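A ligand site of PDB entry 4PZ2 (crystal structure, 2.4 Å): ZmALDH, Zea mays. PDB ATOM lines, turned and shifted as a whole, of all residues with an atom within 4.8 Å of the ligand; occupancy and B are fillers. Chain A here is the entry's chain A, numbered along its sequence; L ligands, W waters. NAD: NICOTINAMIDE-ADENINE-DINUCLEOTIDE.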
ATOM      1  N   ILE A 195      23.191 -26.015  21.159  1.00  0.00           N
ATOM      2  CA  ILE A 195      23.157 -24.553  21.260  1.00  0.00           C
ATOM      3  C   ILE A 195      22.690 -23.986  19.902  1.00  0.00           C
ATOM      4  O   ILE A 195      23.357 -24.173  18.883  1.00  0.00           O
ATOM      5  CB  ILE A 195      24.503 -23.938  21.788  1.00  0.00           C
ATOM      6  CG1 ILE A 195      24.924 -24.546  23.162  1.00  0.00           C
ATOM      7  CG2 ILE A 195      24.379 -22.427  21.909  1.00  0.00           C
ATOM      8  CD1 ILE A 195      26.440 -24.565  23.451  1.00  0.00           C
ATOM      9  N   ILE A 196      21.513 -23.355  19.886  1.00  0.00           N
ATOM     10  CA  ILE A 196      20.886 -22.879  18.640  1.00  0.00           C
ATOM     11  C   ILE A 196      20.492 -21.373  18.604  1.00  0.00           C
ATOM     12  O   ILE A 196      20.379 -20.733  19.667  1.00  0.00           O
ATOM     13  CB  ILE A 196      19.714 -23.824  18.240  1.00  0.00           C
ATOM     14  CG1 ILE A 196      18.868 -24.221  19.492  1.00  0.00           C
ATOM     15  CG2 ILE A 196      20.289 -25.045  17.489  1.00  0.00           C
ATOM     16  CD1 ILE A 196      17.542 -24.809  19.195  1.00  0.00           C
ATOM     17  N   PRO A 197      20.314 -20.786  17.386  1.00  0.00           N
ATOM     18  CA  PRO A 197      19.990 -19.349  17.306  1.00  0.00           C
ATOM     19  C   PRO A 197      18.491 -19.062  17.373  1.00  0.00           C
ATOM     20  O   PRO A 197      17.678 -19.983  17.478  1.00  0.00           O
ATOM     21  CB  PRO A 197      20.612 -18.925  15.976  1.00  0.00           C
ATOM     22  CG  PRO A 197      20.484 -20.129  15.127  1.00  0.00           C
ATOM     23  CD  PRO A 197      20.435 -21.353  16.034  1.00  0.00           C
ATOM     24  N   TRP A 198      18.142 -17.767  17.270  1.00  0.00           N
ATOM     25  CA  TRP A 198      16.792 -17.223  17.389  1.00  0.00           C
ATOM     26  C   TRP A 198      15.970 -17.156  16.116  1.00  0.00           C
ATOM     27  O   TRP A 198      14.754 -16.955  16.209  1.00  0.00           O
ATOM     28  CB  TRP A 198      16.841 -15.843  18.067  1.00  0.00           C
ATOM     29  CG  TRP A 198      17.811 -14.873  17.449  1.00  0.00           C
ATOM     30  CD1 TRP A 198      19.050 -14.555  17.917  1.00  0.00           C
ATOM     31  CD2 TRP A 198      17.641 -14.145  16.228  1.00  0.00           C
ATOM     32  NE1 TRP A 198      19.649 -13.643  17.070  1.00  0.00           N
ATOM     33  CE2 TRP A 198      18.822 -13.394  16.010  1.00  0.00           C
ATOM     34  CE3 TRP A 198      16.601 -14.039  15.278  1.00  0.00           C
ATOM     35  CZ2 TRP A 198      18.993 -12.557  14.897  1.00  0.00           C
ATOM     36  CZ3 TRP A 198      16.777 -13.233  14.166  1.00  0.00           C
ATOM     37  CH2 TRP A 198      17.937 -12.460  14.014  1.00  0.00           C
ATOM     38  N   ASN A 199      16.612 -17.260  14.919  1.00  0.00           N
ATOM     39  CA  ASN A 199      15.930 -17.065  13.639  1.00  0.00           C
ATOM     40  C   ASN A 199      14.915 -18.123  13.208  1.00  0.00           C
ATOM     41  O   ASN A 199      13.900 -17.761  12.612  1.00  0.00           O
ATOM     42  CB  ASN A 199      16.901 -16.691  12.533  1.00  0.00           C
ATOM     43  CG  ASN A 199      17.878 -17.769  12.152  1.00  0.00           C
ATOM     44  OD1 ASN A 199      18.393 -18.506  12.983  1.00  0.00           O
ATOM     45  ND2 ASN A 199      18.190 -17.847  10.874  1.00  0.00           N
ATOM     46  N   PHE A 200      15.201 -19.407  13.471  1.00  0.00           N
ATOM     47  CA  PHE A 200      14.261 -20.485  13.146  1.00  0.00           C
ATOM     48  C   PHE A 200      14.157 -21.366  14.401  1.00  0.00           C
ATOM     49  O   PHE A 200      14.745 -22.444  14.444  1.00  0.00           O
ATOM     50  CB  PHE A 200      14.716 -21.280  11.893  1.00  0.00           C
ATOM     51  CG  PHE A 200      14.971 -20.453  10.655  1.00  0.00           C
ATOM     52  CD1 PHE A 200      13.939 -19.741  10.045  1.00  0.00           C
ATOM     53  CD2 PHE A 200      16.225 -20.430  10.055  1.00  0.00           C
ATOM     54  CE1 PHE A 200      14.172 -18.980   8.902  1.00  0.00           C
ATOM     55  CE2 PHE A 200      16.459 -19.692   8.893  1.00  0.00           C
ATOM     56  CZ  PHE A 200      15.431 -18.964   8.332  1.00  0.00           C
ATOM     57  N   MET A 204      15.236 -25.237  14.234  1.00  0.00           N
ATOM     58  CA  MET A 204      16.528 -25.464  14.901  1.00  0.00           C
ATOM     59  C   MET A 204      16.427 -26.546  15.954  1.00  0.00           C
ATOM     60  O   MET A 204      17.293 -27.437  15.990  1.00  0.00           O
ATOM     61  CB  MET A 204      17.091 -24.156  15.470  1.00  0.00           C
ATOM     62  CG  MET A 204      17.695 -23.250  14.435  1.00  0.00           C
ATOM     63  SD  MET A 204      19.003 -24.075  13.521  1.00  0.00           S
ATOM     64  CE  MET A 204      18.713 -23.385  11.930  1.00  0.00           C
ATOM     65  N   LYS A 222      20.012 -25.674  24.659  1.00  0.00           N
ATOM     66  CA  LYS A 222      20.109 -24.283  25.095  1.00  0.00           C
ATOM     67  C   LYS A 222      19.585 -23.412  23.944  1.00  0.00           C
ATOM     68  O   LYS A 222      20.325 -23.132  23.000  1.00  0.00           O
ATOM     69  CB  LYS A 222      21.538 -23.891  25.507  1.00  0.00           C
ATOM     70  CG  LYS A 222      21.606 -22.864  26.645  1.00  0.00           C
ATOM     71  CD  LYS A 222      21.012 -21.460  26.348  1.00  0.00           C
ATOM     72  CE  LYS A 222      21.834 -20.611  25.396  1.00  0.00           C
ATOM     73  NZ  LYS A 222      21.072 -19.449  24.914  1.00  0.00           N
ATOM     74  N   PRO A 223      18.286 -23.008  24.000  1.00  0.00           N
ATOM     75  CA  PRO A 223      17.758 -22.147  22.923  1.00  0.00           C
ATOM     76  C   PRO A 223      18.203 -20.687  23.096  1.00  0.00           C
ATOM     77  O   PRO A 223      18.558 -20.284  24.213  1.00  0.00           O
ATOM     78  CB  PRO A 223      16.242 -22.288  23.063  1.00  0.00           C
ATOM     79  CG  PRO A 223      16.019 -22.601  24.517  1.00  0.00           C
ATOM     80  CD  PRO A 223      17.271 -23.269  25.045  1.00  0.00           C
ATOM     81  N   ALA A 224      18.183 -19.895  22.006  1.00  0.00           N
ATOM     82  CA  ALA A 224      18.555 -18.490  22.057  1.00  0.00           C
ATOM     83  C   ALA A 224      17.581 -17.727  22.931  1.00  0.00           C
ATOM     84  O   ALA A 224      16.382 -18.006  22.896  1.00  0.00           O
ATOM     85  CB  ALA A 224      18.596 -17.903  20.658  1.00  0.00           C
ATOM     86  N   GLU A 225      18.107 -16.799  23.751  1.00  0.00           N
ATOM     87  CA  GLU A 225      17.367 -15.972  24.714  1.00  0.00           C
ATOM     88  C   GLU A 225      16.303 -15.061  24.105  1.00  0.00           C
ATOM     89  O   GLU A 225      15.347 -14.704  24.791  1.00  0.00           O
ATOM     90  CB  GLU A 225      18.331 -15.188  25.639  1.00  0.00           C
ATOM     91  CG  GLU A 225      19.377 -14.314  24.937  1.00  0.00           C
ATOM     92  CD  GLU A 225      20.707 -14.955  24.602  1.00  0.00           C
ATOM     93  OE1 GLU A 225      20.715 -16.099  24.087  1.00  0.00           O
ATOM     94  OE2 GLU A 225      21.748 -14.305  24.844  1.00  0.00           O
ATOM     95  N   GLN A 226      16.460 -14.704  22.819  1.00  0.00           N
ATOM     96  CA  GLN A 226      15.535 -13.833  22.084  1.00  0.00           C
ATOM     97  C   GLN A 226      14.206 -14.497  21.753  1.00  0.00           C
ATOM     98  O   GLN A 226      13.182 -13.814  21.713  1.00  0.00           O
ATOM     99  CB  GLN A 226      16.193 -13.286  20.796  1.00  0.00           C
ATOM    100  CG  GLN A 226      17.439 -12.433  21.061  1.00  0.00           C
ATOM    101  CD  GLN A 226      18.747 -13.166  20.927  1.00  0.00           C
ATOM    102  OE1 GLN A 226      19.731 -12.582  20.515  1.00  0.00           O
ATOM    103  NE2 GLN A 226      18.789 -14.444  21.223  1.00  0.00           N
ATOM    104  N   GLY A 253      18.379 -19.441  28.533  1.00  0.00           N
ATOM    105  CA  GLY A 253      19.232 -18.519  29.278  1.00  0.00           C
ATOM    106  C   GLY A 253      20.148 -17.754  28.350  1.00  0.00           C
ATOM    107  O   GLY A 253      19.973 -17.771  27.132  1.00  0.00           O
ATOM    108  N   PHE A 254      21.119 -17.069  28.919  1.00  0.00           N
ATOM    109  CA  PHE A 254      22.038 -16.271  28.101  1.00  0.00           C
ATOM    110  C   PHE A 254      23.188 -17.123  27.635  1.00  0.00           C
ATOM    111  O   PHE A 254      23.471 -18.156  28.241  1.00  0.00           O
ATOM    112  CB  PHE A 254      22.492 -15.001  28.858  1.00  0.00           C
ATOM    113  CG  PHE A 254      21.362 -14.097  29.274  1.00  0.00           C
ATOM    114  CD1 PHE A 254      20.609 -13.407  28.322  1.00  0.00           C
ATOM    115  CD2 PHE A 254      21.040 -13.928  30.609  1.00  0.00           C
ATOM    116  CE1 PHE A 254      19.574 -12.565  28.708  1.00  0.00           C
ATOM    117  CE2 PHE A 254      20.007 -13.085  31.004  1.00  0.00           C
ATOM    118  CZ  PHE A 254      19.272 -12.408  30.049  1.00  0.00           C
ATOM    119  N   GLY A 255      23.781 -16.728  26.512  1.00  0.00           N
ATOM    120  CA  GLY A 255      24.899 -17.428  25.917  1.00  0.00           C
ATOM    121  C   GLY A 255      26.126 -17.564  26.800  1.00  0.00           C
ATOM    122  O   GLY A 255      26.508 -18.679  27.149  1.00  0.00           O
ATOM    123  N   PRO A 256      26.746 -16.437  27.236  1.00  0.00           N
ATOM    124  CA  PRO A 256      27.935 -16.547  28.116  1.00  0.00           C
ATOM    125  C   PRO A 256      27.709 -17.230  29.479  1.00  0.00           C
ATOM    126  O   PRO A 256      28.697 -17.548  30.140  1.00  0.00           O
ATOM    127  CB  PRO A 256      28.372 -15.094  28.302  1.00  0.00           C
ATOM    128  CG  PRO A 256      27.754 -14.357  27.176  1.00  0.00           C
ATOM    129  CD  PRO A 256      26.445 -15.033  26.934  1.00  0.00           C
ATOM    130  N   GLY A 259      24.823 -21.126  27.966  1.00  0.00           N
ATOM    131  CA  GLY A 259      25.457 -21.651  26.746  1.00  0.00           C
ATOM    132  C   GLY A 259      26.888 -22.094  26.959  1.00  0.00           C
ATOM    133  O   GLY A 259      27.265 -23.186  26.540  1.00  0.00           O
ATOM    134  N   ALA A 260      27.698 -21.227  27.617  1.00  0.00           N
ATOM    135  CA  ALA A 260      29.108 -21.498  27.945  1.00  0.00           C
ATOM    136  C   ALA A 260      29.250 -22.675  28.911  1.00  0.00           C
ATOM    137  O   ALA A 260      30.183 -23.461  28.745  1.00  0.00           O
ATOM    138  CB  ALA A 260      29.759 -20.253  28.539  1.00  0.00           C
ATOM    139  N   PHE A 273      26.455 -26.873  17.495  1.00  0.00           N
ATOM    140  CA  PHE A 273      26.230 -25.438  17.607  1.00  0.00           C
ATOM    141  C   PHE A 273      25.809 -24.810  16.304  1.00  0.00           C
ATOM    142  O   PHE A 273      26.420 -25.042  15.262  1.00  0.00           O
ATOM    143  CB  PHE A 273      27.488 -24.740  18.182  1.00  0.00           C
ATOM    144  CG  PHE A 273      27.436 -23.220  18.158  1.00  0.00           C
ATOM    145  CD1 PHE A 273      26.750 -22.522  19.149  1.00  0.00           C
ATOM    146  CD2 PHE A 273      28.058 -22.509  17.146  1.00  0.00           C
ATOM    147  CE1 PHE A 273      26.682 -21.123  19.119  1.00  0.00           C
ATOM    148  CE2 PHE A 273      27.988 -21.110  17.106  1.00  0.00           C
ATOM    149  CZ  PHE A 273      27.296 -20.432  18.090  1.00  0.00           C
ATOM    150  N   THR A 274      24.812 -23.941  16.397  1.00  0.00           N
ATOM    151  CA  THR A 274      24.338 -23.112  15.309  1.00  0.00           C
ATOM    152  C   THR A 274      24.293 -21.668  15.808  1.00  0.00           C
ATOM    153  O   THR A 274      23.642 -21.383  16.815  1.00  0.00           O
ATOM    154  CB  THR A 274      23.017 -23.586  14.720  1.00  0.00           C
ATOM    155  OG1 THR A 274      23.170 -24.910  14.265  1.00  0.00           O
ATOM    156  CG2 THR A 274      22.582 -22.741  13.568  1.00  0.00           C
ATOM    157  N   GLY A 275      25.001 -20.798  15.102  1.00  0.00           N
ATOM    158  CA  GLY A 275      25.069 -19.393  15.451  1.00  0.00           C
ATOM    159  C   GLY A 275      26.153 -18.690  14.660  1.00  0.00           C
ATOM    160  O   GLY A 275      26.540 -19.154  13.582  1.00  0.00           O
ATOM    161  N   SER A 276      26.637 -17.559  15.183  1.00  0.00           N
ATOM    162  CA  SER A 276      27.668 -16.759  14.523  1.00  0.00           C
ATOM    163  C   SER A 276      29.049 -17.428  14.509  1.00  0.00           C
ATOM    164  O   SER A 276      29.333 -18.263  15.378  1.00  0.00           O
ATOM    165  CB  SER A 276      27.760 -15.372  15.157  1.00  0.00           C
ATOM    166  OG  SER A 276      28.256 -15.457  16.487  1.00  0.00           O
ATOM    167  N   VAL A 279      31.026 -16.648  17.824  1.00  0.00           N
ATOM    168  CA  VAL A 279      30.635 -17.483  18.984  1.00  0.00           C
ATOM    169  C   VAL A 279      31.155 -18.927  18.796  1.00  0.00           C
ATOM    170  O   VAL A 279      31.538 -19.560  19.777  1.00  0.00           O
ATOM    171  CB  VAL A 279      29.133 -17.370  19.357  1.00  0.00           C
ATOM    172  CG1 VAL A 279      28.740 -18.378  20.439  1.00  0.00           C
ATOM    173  CG2 VAL A 279      28.801 -15.952  19.820  1.00  0.00           C
ATOM    174  N   LEU A 282      34.336 -19.624  20.544  1.00  0.00           N
ATOM    175  CA  LEU A 282      34.137 -19.842  21.973  1.00  0.00           C
ATOM    176  C   LEU A 282      33.679 -21.254  22.308  1.00  0.00           C
ATOM    177  O   LEU A 282      34.038 -21.749  23.377  1.00  0.00           O
ATOM    178  CB  LEU A 282      33.200 -18.773  22.573  1.00  0.00           C
ATOM    179  CG  LEU A 282      33.651 -17.310  22.464  1.00  0.00           C
ATOM    180  CD1 LEU A 282      32.532 -16.366  22.810  1.00  0.00           C
ATOM    181  CD2 LEU A 282      34.826 -17.028  23.345  1.00  0.00           C
ATOM    182  N   ILE A 283      32.919 -21.896  21.411  1.00  0.00           N
ATOM    183  CA  ILE A 283      32.428 -23.277  21.544  1.00  0.00           C
ATOM    184  C   ILE A 283      33.619 -24.235  21.419  1.00  0.00           C
ATOM    185  O   ILE A 283      33.731 -25.195  22.208  1.00  0.00           O
ATOM    186  CB  ILE A 283      31.296 -23.549  20.485  1.00  0.00           C
ATOM    187  CG1 ILE A 283      30.138 -22.498  20.583  1.00  0.00           C
ATOM    188  CG2 ILE A 283      30.760 -24.995  20.532  1.00  0.00           C
ATOM    189  CD1 ILE A 283      29.312 -22.487  21.919  1.00  0.00           C
ATOM    190  N   GLU A 298      27.634 -24.768  12.700  1.00  0.00           N
ATOM    191  CA  GLU A 298      26.740 -24.259  11.666  1.00  0.00           C
ATOM    192  C   GLU A 298      26.790 -22.777  11.878  1.00  0.00           C
ATOM    193  O   GLU A 298      26.158 -22.231  12.786  1.00  0.00           O
ATOM    194  CB  GLU A 298      25.314 -24.805  11.869  1.00  0.00           C
ATOM    195  CG  GLU A 298      25.138 -26.283  11.524  1.00  0.00           C
ATOM    196  CD  GLU A 298      24.934 -26.665  10.064  1.00  0.00           C
ATOM    197  OE1 GLU A 298      25.044 -27.879   9.767  1.00  0.00           O
ATOM    198  OE2 GLU A 298      24.688 -25.772   9.212  1.00  0.00           O
ATOM    199  N   LEU A 299      27.663 -22.116  11.116  1.00  0.00           N
ATOM    200  CA  LEU A 299      27.959 -20.694  11.269  1.00  0.00           C
ATOM    201  C   LEU A 299      27.269 -19.768  10.249  1.00  0.00           C
ATOM    202  O   LEU A 299      26.323 -20.195   9.569  1.00  0.00           O
ATOM    203  CB  LEU A 299      29.493 -20.462  11.386  1.00  0.00           C
ATOM    204  CG  LEU A 299      30.241 -21.428  12.332  1.00  0.00           C
ATOM    205  CD1 LEU A 299      31.728 -21.418  12.097  1.00  0.00           C
ATOM    206  CD2 LEU A 299      29.811 -21.266  13.789  1.00  0.00           C
ATOM    207  N   GLY A 300      27.739 -18.517  10.185  1.00  0.00           N
ATOM    208  CA  GLY A 300      27.163 -17.510   9.305  1.00  0.00           C
ATOM    209  C   GLY A 300      27.406 -17.685   7.825  1.00  0.00           C
ATOM    210  O   GLY A 300      27.986 -18.691   7.386  1.00  0.00           O
ATOM    211  N   GLY A 301      26.985 -16.702   7.041  1.00  0.00           N
ATOM    212  CA  GLY A 301      27.169 -16.749   5.597  1.00  0.00           C
ATOM    213  C   GLY A 301      27.062 -15.433   4.879  1.00  0.00           C
ATOM    214  O   GLY A 301      26.560 -14.445   5.434  1.00  0.00           O
ATOM    215  N   CYS A 332      20.460 -17.554   7.506  1.00  0.00           N
ATOM    216  CA  CYS A 332      21.898 -17.832   7.350  1.00  0.00           C
ATOM    217  C   CYS A 332      22.284 -18.058   5.899  1.00  0.00           C
ATOM    218  O   CYS A 332      23.430 -17.836   5.508  1.00  0.00           O
ATOM    219  CB  CYS A 332      22.235 -19.071   8.178  1.00  0.00           C
ATOM    220  SG  CYS A 332      21.161 -20.509   7.815  1.00  0.00           S
ATOM    221  N   GLU A 432      28.282 -10.238   7.162  1.00  0.00           N
ATOM    222  CA  GLU A 432      26.921 -10.748   7.344  1.00  0.00           C
ATOM    223  C   GLU A 432      26.057  -9.722   8.105  1.00  0.00           C
ATOM    224  O   GLU A 432      26.240  -9.502   9.314  1.00  0.00           O
ATOM    225  CB  GLU A 432      26.912 -12.120   8.025  1.00  0.00           C
ATOM    226  CG  GLU A 432      25.544 -12.763   8.117  1.00  0.00           C
ATOM    227  CD  GLU A 432      25.483 -14.074   8.878  1.00  0.00           C
ATOM    228  OE1 GLU A 432      26.026 -14.111  10.015  1.00  0.00           O
ATOM    229  OE2 GLU A 432      24.870 -15.037   8.375  1.00  0.00           O
ATOM    230  N   PHE A 434      22.539  -9.841   8.196  1.00  0.00           N
ATOM    231  CA  PHE A 434      21.431 -10.580   8.830  1.00  0.00           C
ATOM    232  C   PHE A 434      20.152  -9.717   8.976  1.00  0.00           C
ATOM    233  O   PHE A 434      19.481  -9.721  10.013  1.00  0.00           O
ATOM    234  CB  PHE A 434      21.885 -11.240  10.168  1.00  0.00           C
ATOM    235  CG  PHE A 434      21.283 -12.605  10.433  1.00  0.00           C
ATOM    236  CD1 PHE A 434      21.611 -13.688   9.631  1.00  0.00           C
ATOM    237  CD2 PHE A 434      20.423 -12.808  11.505  1.00  0.00           C
ATOM    238  CE1 PHE A 434      21.063 -14.955   9.863  1.00  0.00           C
ATOM    239  CE2 PHE A 434      19.889 -14.075  11.754  1.00  0.00           C
ATOM    240  CZ  PHE A 434      20.206 -15.137  10.933  1.00  0.00           C
ATOM    241  N   LEU A 460      28.516 -21.267   3.030  1.00  0.00           N
ATOM    242  CA  LEU A 460      27.324 -22.000   3.446  1.00  0.00           C
ATOM    243  C   LEU A 460      26.463 -22.372   2.210  1.00  0.00           C
ATOM    244  O   LEU A 460      26.463 -23.530   1.801  1.00  0.00           O
ATOM    245  CB  LEU A 460      26.536 -21.190   4.527  1.00  0.00           C
ATOM    246  CG  LEU A 460      25.387 -21.930   5.254  1.00  0.00           C
ATOM    247  CD1 LEU A 460      25.862 -23.239   5.886  1.00  0.00           C
ATOM    248  CD2 LEU A 460      24.713 -21.019   6.244  1.00  0.00           C
ATOM    249  N   PHE A 498      22.823 -30.498   5.138  1.00  0.00           N
ATOM    250  CA  PHE A 498      23.083 -29.059   5.216  1.00  0.00           C
ATOM    251  C   PHE A 498      24.225 -28.754   6.156  1.00  0.00           C
ATOM    252  O   PHE A 498      24.159 -29.066   7.352  1.00  0.00           O
ATOM    253  CB  PHE A 498      21.807 -28.285   5.618  1.00  0.00           C
ATOM    254  CG  PHE A 498      21.966 -26.779   5.613  1.00  0.00           C
ATOM    255  CD1 PHE A 498      21.799 -26.044   4.442  1.00  0.00           C
ATOM    256  CD2 PHE A 498      22.287 -26.088   6.777  1.00  0.00           C
ATOM    257  CE1 PHE A 498      21.973 -24.654   4.422  1.00  0.00           C
ATOM    258  CE2 PHE A 498      22.452 -24.705   6.770  1.00  0.00           C
ATOM    259  CZ  PHE A 498      22.288 -23.993   5.590  1.00  0.00           C
HETATM  260  PA  NAD L   1      24.959 -16.126  18.372  1.00  0.00           P
HETATM  261  O1A NAD L   1      26.280 -16.599  17.901  1.00  0.00           O
HETATM  262  O2A NAD L   1      24.991 -14.755  19.034  1.00  0.00           O
HETATM  263  O5B NAD L   1      24.330 -17.165  19.373  1.00  0.00           O
HETATM  264  C5B NAD L   1      23.790 -18.459  19.014  1.00  0.00           C
HETATM  265  C4B NAD L   1      23.530 -19.208  20.298  1.00  0.00           C
HETATM  266  O4B NAD L   1      24.760 -19.280  21.051  1.00  0.00           O
HETATM  267  C3B NAD L   1      22.484 -18.637  21.249  1.00  0.00           C
HETATM  268  O3B NAD L   1      21.757 -19.676  21.892  1.00  0.00           O
HETATM  269  C2B NAD L   1      23.319 -17.861  22.260  1.00  0.00           C
HETATM  270  O2B NAD L   1      22.661 -17.705  23.518  1.00  0.00           O
HETATM  271  C1B NAD L   1      24.556 -18.757  22.356  1.00  0.00           C
HETATM  272  N9A NAD L   1      25.791 -18.132  22.808  1.00  0.00           N
HETATM  273  C8A NAD L   1      26.154 -16.815  22.724  1.00  0.00           C
HETATM  274  N7A NAD L   1      27.288 -16.534  23.306  1.00  0.00           N
HETATM  275  C5A NAD L   1      27.728 -17.766  23.774  1.00  0.00           C
HETATM  276  C6A NAD L   1      28.913 -18.159  24.441  1.00  0.00           C
HETATM  277  N6A NAD L   1      29.873 -17.302  24.821  1.00  0.00           N
HETATM  278  N1A NAD L   1      29.070 -19.469  24.720  1.00  0.00           N
HETATM  279  C2A NAD L   1      28.098 -20.319  24.374  1.00  0.00           C
HETATM  280  N3A NAD L   1      26.931 -20.065  23.765  1.00  0.00           N
HETATM  281  C4A NAD L   1      26.823 -18.755  23.473  1.00  0.00           C
HETATM  282  O3  NAD L   1      23.955 -16.055  17.125  1.00  0.00           O
HETATM  283  PN  NAD L   1      22.436 -15.581  16.953  1.00  0.00           P
HETATM  284  O1N NAD L   1      22.453 -14.101  16.946  1.00  0.00           O
HETATM  285  O2N NAD L   1      21.589 -16.288  17.941  1.00  0.00           O
HETATM  286  O5D NAD L   1      22.039 -16.171  15.521  1.00  0.00           O
HETATM  287  C5D NAD L   1      22.398 -15.514  14.291  1.00  0.00           C
HETATM  288  C4D NAD L   1      23.553 -16.255  13.669  1.00  0.00           C
HETATM  289  O4D NAD L   1      23.169 -17.633  13.421  1.00  0.00           O
HETATM  290  C3D NAD L   1      24.022 -15.735  12.319  1.00  0.00           C
HETATM  291  O3D NAD L   1      25.445 -15.634  12.301  1.00  0.00           O
HETATM  292  C2D NAD L   1      23.495 -16.804  11.356  1.00  0.00           C
HETATM  293  O2D NAD L   1      24.214 -16.974  10.145  1.00  0.00           O
HETATM  294  C1D NAD L   1      23.626 -18.097  12.200  1.00  0.00           C
HETATM  295  N1N NAD L   1      22.699 -19.183  11.676  1.00  0.00           N
HETATM  296  C2N NAD L   1      23.355 -20.286  11.070  1.00  0.00           C
HETATM  297  C3N NAD L   1      22.604 -21.363  10.612  1.00  0.00           C
HETATM  298  C7N NAD L   1      23.231 -22.535   9.906  1.00  0.00           C
HETATM  299  O7N NAD L   1      24.424 -22.481   9.547  1.00  0.00           O
HETATM  300  N7N NAD L   1      22.443 -23.546   9.587  1.00  0.00           N
HETATM  301  C4N NAD L   1      21.218 -21.312  10.743  1.00  0.00           C
HETATM  302  C5N NAD L   1      20.594 -20.200  11.298  1.00  0.00           C
HETATM  303  C6N NAD L   1      21.354 -19.144  11.765  1.00  0.00           C
HETATM  304  O   HOH W   1      21.056 -15.640  20.545  1.00  0.00           O
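An oxygen (O2B) of the ligand lies close to the backbone NH (N) of Gly 255, at 3.3 Å.
A nitrogen (N7N) of the ligand lies within hydrogen-bond range of the side-chain carboxylate of Glu 298.
An oxygen (O1A) of the ligand sits at hydrogen-bond distance from the backbone NH (N) of Ser 276 (2.9 Å).
OE1 of Glu 225 is in hydrogen-bond range of O2B of the ligand (2.6 Å).
NE1 of Trp 198 lies within hydrogen-bond range of O1N of the ligand, 2.8 Å away.
The side-chain amino group (NZ) of Lys 222 is in hydrogen-bond range of an oxygen (O2B) of the ligand, at 2.7 Å.
The side-chain hydroxyl (OG) of Ser 276 sits at hydrogen-bond distance from an oxygen (O1A) of the ligand (2.7 Å).
The side-chain sulfur of Cys 332 sits close to a nitrogen (N7N) of the ligand.
O2D of the ligand lies within hydrogen-bond range of OE2 of Glu 432, at 2.7 Å.
The backbone carbonyl oxygen (O) of Ile 196 is in hydrogen-bond range of an oxygen (O3B) of the ligand, at 2.8 Å.
The backbone NH of Thr 274 lies within hydrogen-bond range of the backbone carbonyl oxygen of Ile 195, 2.9 Å away.
NZ of Lys 222 sits at hydrogen-bond distance from O of Gly 253 (3.0 Å).
O of Glu 298 sits at hydrogen-bond distance from N of Gly 275 (3.0 Å).
O of Phe 273 sits at hydrogen-bond distance from N of Glu 298, 2.8 Å away.
NZ of Lys 222 is in salt-bridge range of OE1 of Glu 225 (3.5 Å).
O of Ile 196 is in hydrogen-bond range of N of Ala 224 (3.3 Å).
The backbone NH (N) of Val 279 is in hydrogen-bond range of the side-chain hydroxyl (OG) of Ser 276 (3.3 Å).
The backbone carbonyl oxygen of Phe 254 sits at hydrogen-bond distance from the backbone NH of Gly 259, 3.3 Å away.
The backbone carbonyl oxygen (O) of Leu 299 sits close to an oxygen (O7N) of the ligand (3.0 Å).
CG2 of Ile 195 touches O4B of the ligand (3.3 Å).
Pro 197 touches the ligand (CB to O5D, 3.1 Å).
Asn 199 touches the ligand (OD1 to C5N, 3.2 Å).
Met 204 touches the ligand.
Pro 223 touches the ligand (C to O3B, 3.9 Å).
CA of Ala 224 touches O3B of the ligand, 3.4 Å away.
Pro 256 touches the ligand.
C of Gly 259 touches C2A of the ligand, 3.4 Å away.
Ala 260 touches the ligand.
Phe 273 touches the ligand (CE1 to O4B, 3.3 Å).
Thr 274 touches the ligand (CG2 to C3N, 3.3 Å).
CA of Gly 275 touches O4D of the ligand (3.3 Å).
Val 279 touches the ligand.
Leu 282 touches the ligand (CD1 to N6A, 3.5 Å).
CD1 of Ile 283 touches C2A of the ligand (3.5 Å).
Gly 300 touches the ligand (CA to O2D, 3.1 Å).
Phe 434 touches the ligand.
Leu 460 touches the ligand.
Phe 498 touches the ligand (CE2 to N7N, 3.0 Å).
Hydrophobic or aromatic side chains within 4 Å of the ligand: Ile 195, Pro 197, Trp 198, Met 204, Ala 224, Ala 260, Phe 273, Val 279, Leu 282, Ile 283, Phe 434, Leu 460 and Phe 498.
Within 4 Å of the ligand: Ile 195, Ile 196, Pro 197, Trp 198, Asn 199, Met 204, Lys 222, Pro 223, Ala 224, Glu 225, Gly 255, Pro 256, Gly 259, Ala 260, Phe 273, Thr 274, Gly 275, Ser 276, Val 279, Leu 282, Ile 283, Glu 298, Leu 299, Gly 300, Cys 332, Glu 432, Phe 434, Leu 460 and Phe 498.
The nearest printed residue that does not touch the ligand is Gly 301 (4.2 Å).
Water W1 lies within hydrogen-bond range of NE2 of Gln 226 (2.7 Å) and O2N of the ligand (2.7 Å).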
